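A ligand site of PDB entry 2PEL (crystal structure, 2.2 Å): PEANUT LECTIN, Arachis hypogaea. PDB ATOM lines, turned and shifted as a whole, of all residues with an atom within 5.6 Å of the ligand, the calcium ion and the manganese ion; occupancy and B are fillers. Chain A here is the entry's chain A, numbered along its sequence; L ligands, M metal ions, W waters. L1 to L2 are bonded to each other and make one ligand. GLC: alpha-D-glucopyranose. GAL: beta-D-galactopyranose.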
ATOM      1  N   ASP A  80      -5.863 -31.347  13.921  1.00  0.00           N
ATOM      2  CA  ASP A  80      -4.859 -31.613  14.946  1.00  0.00           C
ATOM      3  C   ASP A  80      -5.541 -31.372  16.306  1.00  0.00           C
ATOM      4  O   ASP A  80      -5.977 -30.231  16.499  1.00  0.00           O
ATOM      5  CB  ASP A  80      -3.703 -30.629  14.873  1.00  0.00           C
ATOM      6  CG  ASP A  80      -2.627 -30.954  13.868  1.00  0.00           C
ATOM      7  OD1 ASP A  80      -2.894 -31.581  12.800  1.00  0.00           O
ATOM      8  OD2 ASP A  80      -1.473 -30.587  14.151  1.00  0.00           O
ATOM      9  N   ALA A  82      -6.067 -29.997  19.275  1.00  0.00           N
ATOM     10  CA  ALA A  82      -5.511 -28.861  20.038  1.00  0.00           C
ATOM     11  C   ALA A  82      -6.674 -28.034  20.544  1.00  0.00           C
ATOM     12  O   ALA A  82      -7.804 -28.134  20.045  1.00  0.00           O
ATOM     13  CB  ALA A  82      -4.528 -28.133  19.152  1.00  0.00           C
ATOM     14  N   ASP A  83      -6.518 -27.211  21.565  1.00  0.00           N
ATOM     15  CA  ASP A  83      -5.296 -26.935  22.309  1.00  0.00           C
ATOM     16  C   ASP A  83      -5.327 -27.366  23.774  1.00  0.00           C
ATOM     17  O   ASP A  83      -4.244 -27.418  24.373  1.00  0.00           O
ATOM     18  CB  ASP A  83      -5.099 -25.407  22.168  1.00  0.00           C
ATOM     19  CG  ASP A  83      -4.253 -25.069  20.950  1.00  0.00           C
ATOM     20  OD1 ASP A  83      -3.006 -25.035  21.013  1.00  0.00           O
ATOM     21  OD2 ASP A  83      -4.880 -24.834  19.894  1.00  0.00           O
ATOM     22  N   GLY A 103      -5.855 -20.687  20.136  1.00  0.00           N
ATOM     23  CA  GLY A 103      -4.659 -21.505  20.176  1.00  0.00           C
ATOM     24  C   GLY A 103      -4.116 -21.753  21.582  1.00  0.00           C
ATOM     25  O   GLY A 103      -4.833 -22.053  22.535  1.00  0.00           O
ATOM     26  N   GLY A 104      -2.785 -21.609  21.661  1.00  0.00           N
ATOM     27  CA  GLY A 104      -1.971 -21.823  22.844  1.00  0.00           C
ATOM     28  C   GLY A 104      -2.125 -20.842  23.986  1.00  0.00           C
ATOM     29  O   GLY A 104      -1.411 -20.984  25.008  1.00  0.00           O
ATOM     30  N   LEU A 106      -5.012 -20.454  25.297  1.00  0.00           N
ATOM     31  CA  LEU A 106      -6.087 -21.171  25.975  1.00  0.00           C
ATOM     32  C   LEU A 106      -7.308 -20.328  26.348  1.00  0.00           C
ATOM     33  O   LEU A 106      -8.089 -20.647  27.275  1.00  0.00           O
ATOM     34  CB  LEU A 106      -5.460 -21.914  27.190  1.00  0.00           C
ATOM     35  CG  LEU A 106      -4.360 -22.936  26.896  1.00  0.00           C
ATOM     36  CD1 LEU A 106      -3.757 -23.534  28.167  1.00  0.00           C
ATOM     37  CD2 LEU A 106      -4.930 -24.088  26.050  1.00  0.00           C
ATOM     38  N   GLU A 121      -3.630 -26.136  33.704  1.00  0.00           N
ATOM     39  CA  GLU A 121      -3.894 -26.467  32.276  1.00  0.00           C
ATOM     40  C   GLU A 121      -3.657 -27.928  31.893  1.00  0.00           C
ATOM     41  O   GLU A 121      -2.811 -28.646  32.450  1.00  0.00           O
ATOM     42  CB  GLU A 121      -2.983 -25.625  31.389  1.00  0.00           C
ATOM     43  CG  GLU A 121      -1.490 -25.730  31.647  1.00  0.00           C
ATOM     44  CD  GLU A 121      -0.680 -25.072  30.567  1.00  0.00           C
ATOM     45  OE1 GLU A 121      -0.564 -23.857  30.583  1.00  0.00           O
ATOM     46  OE2 GLU A 121      -0.226 -25.846  29.708  1.00  0.00           O
ATOM     47  N   ASP A 123      -2.763 -29.238  28.800  1.00  0.00           N
ATOM     48  CA  ASP A 123      -2.288 -28.788  27.467  1.00  0.00           C
ATOM     49  C   ASP A 123      -1.948 -29.895  26.485  1.00  0.00           C
ATOM     50  O   ASP A 123      -0.985 -30.620  26.747  1.00  0.00           O
ATOM     51  CB  ASP A 123      -1.166 -27.801  27.751  1.00  0.00           C
ATOM     52  CG  ASP A 123      -0.751 -26.964  26.577  1.00  0.00           C
ATOM     53  OD1 ASP A 123      -1.028 -27.293  25.397  1.00  0.00           O
ATOM     54  OD2 ASP A 123      -0.114 -25.918  26.817  1.00  0.00           O
ATOM     55  N   THR A 124      -2.699 -29.952  25.378  1.00  0.00           N
ATOM     56  CA  THR A 124      -2.462 -30.992  24.368  1.00  0.00           C
ATOM     57  C   THR A 124      -1.689 -30.587  23.130  1.00  0.00           C
ATOM     58  O   THR A 124      -1.696 -31.377  22.152  1.00  0.00           O
ATOM     59  CB  THR A 124      -3.801 -31.665  23.872  1.00  0.00           C
ATOM     60  OG1 THR A 124      -4.422 -30.707  22.961  1.00  0.00           O
ATOM     61  CG2 THR A 124      -4.725 -32.095  25.004  1.00  0.00           C
ATOM     62  N   TYR A 125      -1.061 -29.439  23.108  1.00  0.00           N
ATOM     63  CA  TYR A 125      -0.315 -29.026  21.892  1.00  0.00           C
ATOM     64  C   TYR A 125       0.919 -28.272  22.363  1.00  0.00           C
ATOM     65  O   TYR A 125       0.770 -27.386  23.220  1.00  0.00           O
ATOM     66  CB  TYR A 125      -1.154 -28.165  20.915  1.00  0.00           C
ATOM     67  CG  TYR A 125      -0.263 -27.778  19.743  1.00  0.00           C
ATOM     68  CD1 TYR A 125       0.513 -26.602  19.814  1.00  0.00           C
ATOM     69  CD2 TYR A 125      -0.162 -28.606  18.621  1.00  0.00           C
ATOM     70  CE1 TYR A 125       1.374 -26.273  18.777  1.00  0.00           C
ATOM     71  CE2 TYR A 125       0.697 -28.274  17.570  1.00  0.00           C
ATOM     72  CZ  TYR A 125       1.443 -27.101  17.646  1.00  0.00           C
ATOM     73  OH  TYR A 125       2.295 -26.734  16.635  1.00  0.00           O
ATOM     74  N   SER A 126       2.057 -28.535  21.761  1.00  0.00           N
ATOM     75  CA  SER A 126       3.289 -27.856  22.185  1.00  0.00           C
ATOM     76  C   SER A 126       3.643 -26.579  21.457  1.00  0.00           C
ATOM     77  O   SER A 126       4.122 -26.635  20.306  1.00  0.00           O
ATOM     78  CB  SER A 126       4.390 -28.914  22.090  1.00  0.00           C
ATOM     79  OG  SER A 126       5.584 -28.435  22.690  1.00  0.00           O
ATOM     80  N   ASN A 127       3.459 -25.462  22.140  1.00  0.00           N
ATOM     81  CA  ASN A 127       3.729 -24.111  21.650  1.00  0.00           C
ATOM     82  C   ASN A 127       5.099 -23.679  22.184  1.00  0.00           C
ATOM     83  O   ASN A 127       5.196 -23.356  23.379  1.00  0.00           O
ATOM     84  CB  ASN A 127       2.694 -23.062  22.085  1.00  0.00           C
ATOM     85  CG  ASN A 127       1.299 -23.449  21.656  1.00  0.00           C
ATOM     86  OD1 ASN A 127       0.641 -24.175  22.427  1.00  0.00           O
ATOM     87  ND2 ASN A 127       0.797 -23.022  20.500  1.00  0.00           N
ATOM     88  N   GLU A 129       6.533 -21.015  21.617  1.00  0.00           N
ATOM     89  CA  GLU A 129       6.521 -19.596  21.925  1.00  0.00           C
ATOM     90  C   GLU A 129       6.224 -19.394  23.400  1.00  0.00           C
ATOM     91  O   GLU A 129       6.682 -18.363  23.922  1.00  0.00           O
ATOM     92  CB  GLU A 129       5.555 -18.751  21.129  1.00  0.00           C
ATOM     93  CG  GLU A 129       4.067 -19.089  21.037  1.00  0.00           C
ATOM     94  CD  GLU A 129       3.720 -20.204  20.091  1.00  0.00           C
ATOM     95  OE1 GLU A 129       4.726 -20.811  19.636  1.00  0.00           O
ATOM     96  OE2 GLU A 129       2.557 -20.478  19.810  1.00  0.00           O
ATOM     97  N   TYR A 130       5.520 -20.337  23.980  1.00  0.00           N
ATOM     98  CA  TYR A 130       5.196 -20.243  25.419  1.00  0.00           C
ATOM     99  C   TYR A 130       6.001 -21.305  26.169  1.00  0.00           C
ATOM    100  O   TYR A 130       5.555 -21.724  27.243  1.00  0.00           O
ATOM    101  CB  TYR A 130       3.701 -20.426  25.694  1.00  0.00           C
ATOM    102  CG  TYR A 130       2.865 -19.560  24.784  1.00  0.00           C
ATOM    103  CD1 TYR A 130       3.051 -18.182  24.773  1.00  0.00           C
ATOM    104  CD2 TYR A 130       1.915 -20.115  23.927  1.00  0.00           C
ATOM    105  CE1 TYR A 130       2.276 -17.361  23.943  1.00  0.00           C
ATOM    106  CE2 TYR A 130       1.134 -19.326  23.106  1.00  0.00           C
ATOM    107  CZ  TYR A 130       1.315 -17.947  23.118  1.00  0.00           C
ATOM    108  OH  TYR A 130       0.585 -17.143  22.304  1.00  0.00           O
ATOM    109  N   ASP A 132       6.495 -24.524  25.832  1.00  0.00           N
ATOM    110  CA  ASP A 132       5.839 -25.758  26.242  1.00  0.00           C
ATOM    111  C   ASP A 132       6.775 -26.961  26.223  1.00  0.00           C
ATOM    112  O   ASP A 132       7.634 -27.022  25.344  1.00  0.00           O
ATOM    113  CB  ASP A 132       4.739 -26.052  25.221  1.00  0.00           C
ATOM    114  CG  ASP A 132       3.380 -25.489  25.631  1.00  0.00           C
ATOM    115  OD1 ASP A 132       3.262 -25.049  26.782  1.00  0.00           O
ATOM    116  OD2 ASP A 132       2.577 -25.551  24.676  1.00  0.00           O
ATOM    117  N   PRO A 133       6.535 -27.899  27.141  1.00  0.00           N
ATOM    118  CA  PRO A 133       7.300 -29.151  27.162  1.00  0.00           C
ATOM    119  C   PRO A 133       6.913 -29.824  25.819  1.00  0.00           C
ATOM    120  O   PRO A 133       5.877 -29.517  25.175  1.00  0.00           O
ATOM    121  CB  PRO A 133       6.792 -29.888  28.381  1.00  0.00           C
ATOM    122  CG  PRO A 133       6.141 -28.807  29.231  1.00  0.00           C
ATOM    123  CD  PRO A 133       5.520 -27.889  28.190  1.00  0.00           C
ATOM    124  N   HIS A 137       0.799 -32.299  28.636  1.00  0.00           N
ATOM    125  CA  HIS A 137       1.181 -32.002  30.022  1.00  0.00           C
ATOM    126  C   HIS A 137       0.170 -31.235  30.853  1.00  0.00           C
ATOM    127  O   HIS A 137      -0.748 -30.634  30.284  1.00  0.00           O
ATOM    128  CB  HIS A 137       2.512 -31.183  30.027  1.00  0.00           C
ATOM    129  CG  HIS A 137       2.400 -29.935  29.201  1.00  0.00           C
ATOM    130  ND1 HIS A 137       2.459 -29.938  27.812  1.00  0.00           N
ATOM    131  CD2 HIS A 137       2.235 -28.636  29.604  1.00  0.00           C
ATOM    132  CE1 HIS A 137       2.348 -28.688  27.410  1.00  0.00           C
ATOM    133  NE2 HIS A 137       2.213 -27.892  28.450  1.00  0.00           N
ATOM    134  N   VAL A 145       0.873 -18.325  30.255  1.00  0.00           N
ATOM    135  CA  VAL A 145       0.716 -19.710  29.783  1.00  0.00           C
ATOM    136  C   VAL A 145       2.123 -20.351  29.685  1.00  0.00           C
ATOM    137  O   VAL A 145       2.322 -21.468  29.178  1.00  0.00           O
ATOM    138  CB  VAL A 145      -0.086 -19.908  28.497  1.00  0.00           C
ATOM    139  CG1 VAL A 145      -1.592 -19.899  28.761  1.00  0.00           C
ATOM    140  CG2 VAL A 145       0.397 -18.952  27.418  1.00  0.00           C
ATOM    141  N   SER A 147       4.124 -21.768  31.881  1.00  0.00           N
ATOM    142  CA  SER A 147       3.983 -22.434  33.185  1.00  0.00           C
ATOM    143  C   SER A 147       5.242 -22.366  34.065  1.00  0.00           C
ATOM    144  O   SER A 147       6.410 -22.545  33.715  1.00  0.00           O
ATOM    145  CB  SER A 147       3.515 -23.866  33.090  1.00  0.00           C
ATOM    146  OG  SER A 147       2.323 -24.068  32.378  1.00  0.00           O
ATOM    147  N   THR A 150       5.551 -27.729  35.146  1.00  0.00           N
ATOM    148  CA  THR A 150       4.771 -28.697  34.368  1.00  0.00           C
ATOM    149  C   THR A 150       5.211 -30.132  34.676  1.00  0.00           C
ATOM    150  O   THR A 150       6.288 -30.390  35.189  1.00  0.00           O
ATOM    151  CB  THR A 150       4.905 -28.455  32.806  1.00  0.00           C
ATOM    152  OG1 THR A 150       6.284 -28.905  32.560  1.00  0.00           O
ATOM    153  CG2 THR A 150       4.630 -27.029  32.341  1.00  0.00           C
ATOM    154  N   GLY A 210      -8.954 -23.322  20.360  1.00  0.00           N
ATOM    155  CA  GLY A 210      -8.511 -24.001  19.125  1.00  0.00           C
ATOM    156  C   GLY A 210      -7.979 -22.943  18.142  1.00  0.00           C
ATOM    157  O   GLY A 210      -7.976 -21.733  18.471  1.00  0.00           O
ATOM    158  N   SER A 211      -7.506 -23.356  16.987  1.00  0.00           N
ATOM    159  CA  SER A 211      -6.989 -22.434  15.960  1.00  0.00           C
ATOM    160  C   SER A 211      -7.579 -22.894  14.631  1.00  0.00           C
ATOM    161  O   SER A 211      -8.596 -23.607  14.613  1.00  0.00           O
ATOM    162  CB  SER A 211      -5.475 -22.391  15.982  1.00  0.00           C
ATOM    163  OG  SER A 211      -4.838 -23.646  15.762  1.00  0.00           O
ATOM    164  N   LEU A 212      -6.976 -22.487  13.519  1.00  0.00           N
ATOM    165  CA  LEU A 212      -7.471 -22.991  12.181  1.00  0.00           C
ATOM    166  C   LEU A 212      -7.160 -24.409  12.046  1.00  0.00           C
ATOM    167  O   LEU A 212      -8.065 -25.111  11.605  1.00  0.00           O
ATOM    168  CB  LEU A 212      -6.897 -22.109  11.006  1.00  0.00           C
ATOM    169  CG  LEU A 212      -7.345 -22.174   9.556  1.00  0.00           C
ATOM    170  CD1 LEU A 212      -6.603 -21.194   8.664  1.00  0.00           C
ATOM    171  CD2 LEU A 212      -7.098 -23.563   8.950  1.00  0.00           C
ATOM    172  N   GLY A 213      -5.987 -24.932  12.332  1.00  0.00           N
ATOM    173  CA  GLY A 213      -5.712 -26.349  12.011  1.00  0.00           C
ATOM    174  C   GLY A 213      -5.965 -27.177  13.182  1.00  0.00           C
ATOM    175  O   GLY A 213      -6.164 -28.415  13.097  1.00  0.00           O
ATOM    176  N   GLY A 214      -5.851 -26.569  14.353  1.00  0.00           N
ATOM    177  CA  GLY A 214      -5.989 -27.310  15.632  1.00  0.00           C
ATOM    178  C   GLY A 214      -7.389 -27.198  16.232  1.00  0.00           C
ATOM    179  O   GLY A 214      -7.807 -26.117  16.696  1.00  0.00           O
HETATM  180  C1  GLC L   1      -1.177 -21.948  10.496  1.00  0.00           C
HETATM  181  C2  GLC L   1      -2.099 -23.085  10.906  1.00  0.00           C
HETATM  182  C3  GLC L   1      -2.597 -22.809  12.338  1.00  0.00           C
HETATM  183  C4  GLC L   1      -1.358 -22.767  13.260  1.00  0.00           C
HETATM  184  C5  GLC L   1      -0.391 -21.692  12.789  1.00  0.00           C
HETATM  185  C6  GLC L   1       0.937 -21.627  13.497  1.00  0.00           C
HETATM  186  O1  GLC L   1      -2.074 -20.784  10.594  1.00  0.00           O
HETATM  187  O2  GLC L   1      -3.161 -23.164   9.876  1.00  0.00           O
HETATM  188  O3  GLC L   1      -3.278 -23.954  12.826  1.00  0.00           O
HETATM  189  O4  GLC L   1      -1.810 -22.694  14.611  1.00  0.00           O
HETATM  190  O5  GLC L   1      -0.110 -21.872  11.397  1.00  0.00           O
HETATM  191  O6  GLC L   1       1.666 -22.888  13.434  1.00  0.00           O
HETATM  192  C1  GAL L   2      -1.289 -23.570  15.579  1.00  0.00           C
HETATM  193  C2  GAL L   2      -1.642 -22.945  16.931  1.00  0.00           C
HETATM  194  C3  GAL L   2      -1.500 -23.930  18.052  1.00  0.00           C
HETATM  195  C4  GAL L   2      -2.266 -25.205  17.769  1.00  0.00           C
HETATM  196  C5  GAL L   2      -1.726 -25.765  16.459  1.00  0.00           C
HETATM  197  C6  GAL L   2      -2.414 -27.016  16.009  1.00  0.00           C
HETATM  198  O2  GAL L   2      -0.930 -21.766  17.150  1.00  0.00           O
HETATM  199  O3  GAL L   2      -1.793 -23.348  19.328  1.00  0.00           O
HETATM  200  O4  GAL L   2      -3.690 -25.098  17.607  1.00  0.00           O
HETATM  201  O5  GAL L   2      -1.957 -24.800  15.398  1.00  0.00           O
HETATM  202  O6  GAL L   2      -1.892 -27.338  14.732  1.00  0.00           O
HETATM  203 CA    CA M   1       0.202 -25.401  24.435  1.00  0.00          CA
HETATM  204 MN    MN M   2       1.618 -25.614  28.306  1.00  0.00          MN
HETATM  205  O   HOH W   1       3.091 -24.926  29.980  1.00  0.00           O
HETATM  206  O   HOH W   2      -1.515 -20.205  19.173  1.00  0.00           O
HETATM  207  O   HOH W   3       2.021 -22.113  17.307  1.00  0.00           O
HETATM  208  O   HOH W   4      -0.010 -23.307  25.642  1.00  0.00           O
HETATM  209  O   HOH W   5      -2.049 -25.616  23.587  1.00  0.00           O
HETATM  210  O   HOH W   6       0.786 -23.474  28.135  1.00  0.00           O
HETATM  211  O   HOH W   7      -2.507 -19.624  15.410  1.00  0.00           O
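The side-chain amide nitrogen (ND2) of Asn 127 is in hydrogen-bond range of an oxygen (O3) of GAL L2, 2.9 Å away. OD2 of Asp 83 sits at hydrogen-bond distance from O4 of GAL L2 (2.6 Å). The side-chain hydroxyl of Ser 211 is in hydrogen-bond range of an oxygen (O4) of GAL L2. O3 of GLC L1 lies within hydrogen-bond range of N of Gly 213 (2.9 Å). An oxygen (O3) of GAL L2 sits at hydrogen-bond distance from the backbone NH (N) of Gly 104 (3.1 Å). O6 of GAL L2 sits at hydrogen-bond distance from OD2 of Asp 80 (3.3 Å).
The side-chain hydroxyl (OG) of Ser 147 lies within hydrogen-bond range of the side-chain carboxylate (OE1) of Glu 121 (3.4 Å). The side-chain carboxylate of Glu 129 is in hydrogen-bond range of the side-chain amide nitrogen of Asn 127 (3.2 Å). The backbone NH (N) of Gly 104 sits at hydrogen-bond distance from the side-chain carboxylate (OD1) of Asp 83 (3.5 Å). N of Thr 124 is in hydrogen-bond range of O of Asp 83, 3.1 Å away. The side-chain hydroxyl (OG) of Ser 211 sits at hydrogen-bond distance from the backbone NH (N) of Gly 214 (3.4 Å). The backbone NH (N) of Asp 80 is in hydrogen-bond range of the backbone carbonyl oxygen (O) of Gly 213. The backbone carbonyl oxygen (O) of Gly 210 is in hydrogen-bond range of the backbone NH (N) of Gly 103.
Residues that only touch the ligand: Ala 82 (3.5 Å), Gly 103 (3.5 Å), Gly 214 (3.6 Å) and Leu 212 (3.99 Å). Hydrophobic or aromatic side chains within 4 Å of the ligand: Ala 82 and Tyr 125. Of the 25 residues printed, 11 come within 4 Å of the ligand.
Four residues have an atom within 4 Å of the calcium ion: Asp 123, Tyr 125, Asn 127 and Asp 132. Along chain A the residues within 4 Å of the calcium ion span positions 123 to 132.
Of the 25 residues printed, 4 come within 4 Å of the manganese ion.
The calcium ion is bound by OD2 of Asp 132 (2.4 Å), OD1 of Asn 127 (2.4 Å), O of Tyr 125 (2.4 Å), water W5 (2.4 Å), water W4 (2.4 Å), OD1 of Asp 123 (2.5 Å) and OD2 of Asp 123 (2.5 Å). The calcium ion has seven donor atoms within binding distance.
The manganese ion is bound by water W6 (2.3 Å), OD2 of Asp 123 (2.3 Å), OD1 of Asp 132 (2.3 Å), OE2 of Glu 121 (2.3 Å), water W1 (2.3 Å) and NE2 of His 137 (2.4 Å). The manganese ion has six donor atoms within binding distance.
Water W6 lies within hydrogen-bond range of O of Val 145 (2.7 Å) and OE1 of Glu 121 (2.8 Å). Water W2 lies within hydrogen-bond range of an oxygen (O2) of GAL L2 (2.6 Å) and the backbone NH of Gly 104 (3.1 Å). Water W3 bridges O2 of GAL L2 (3.0 Å) and OE2 of Glu 129 (3.0 Å).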
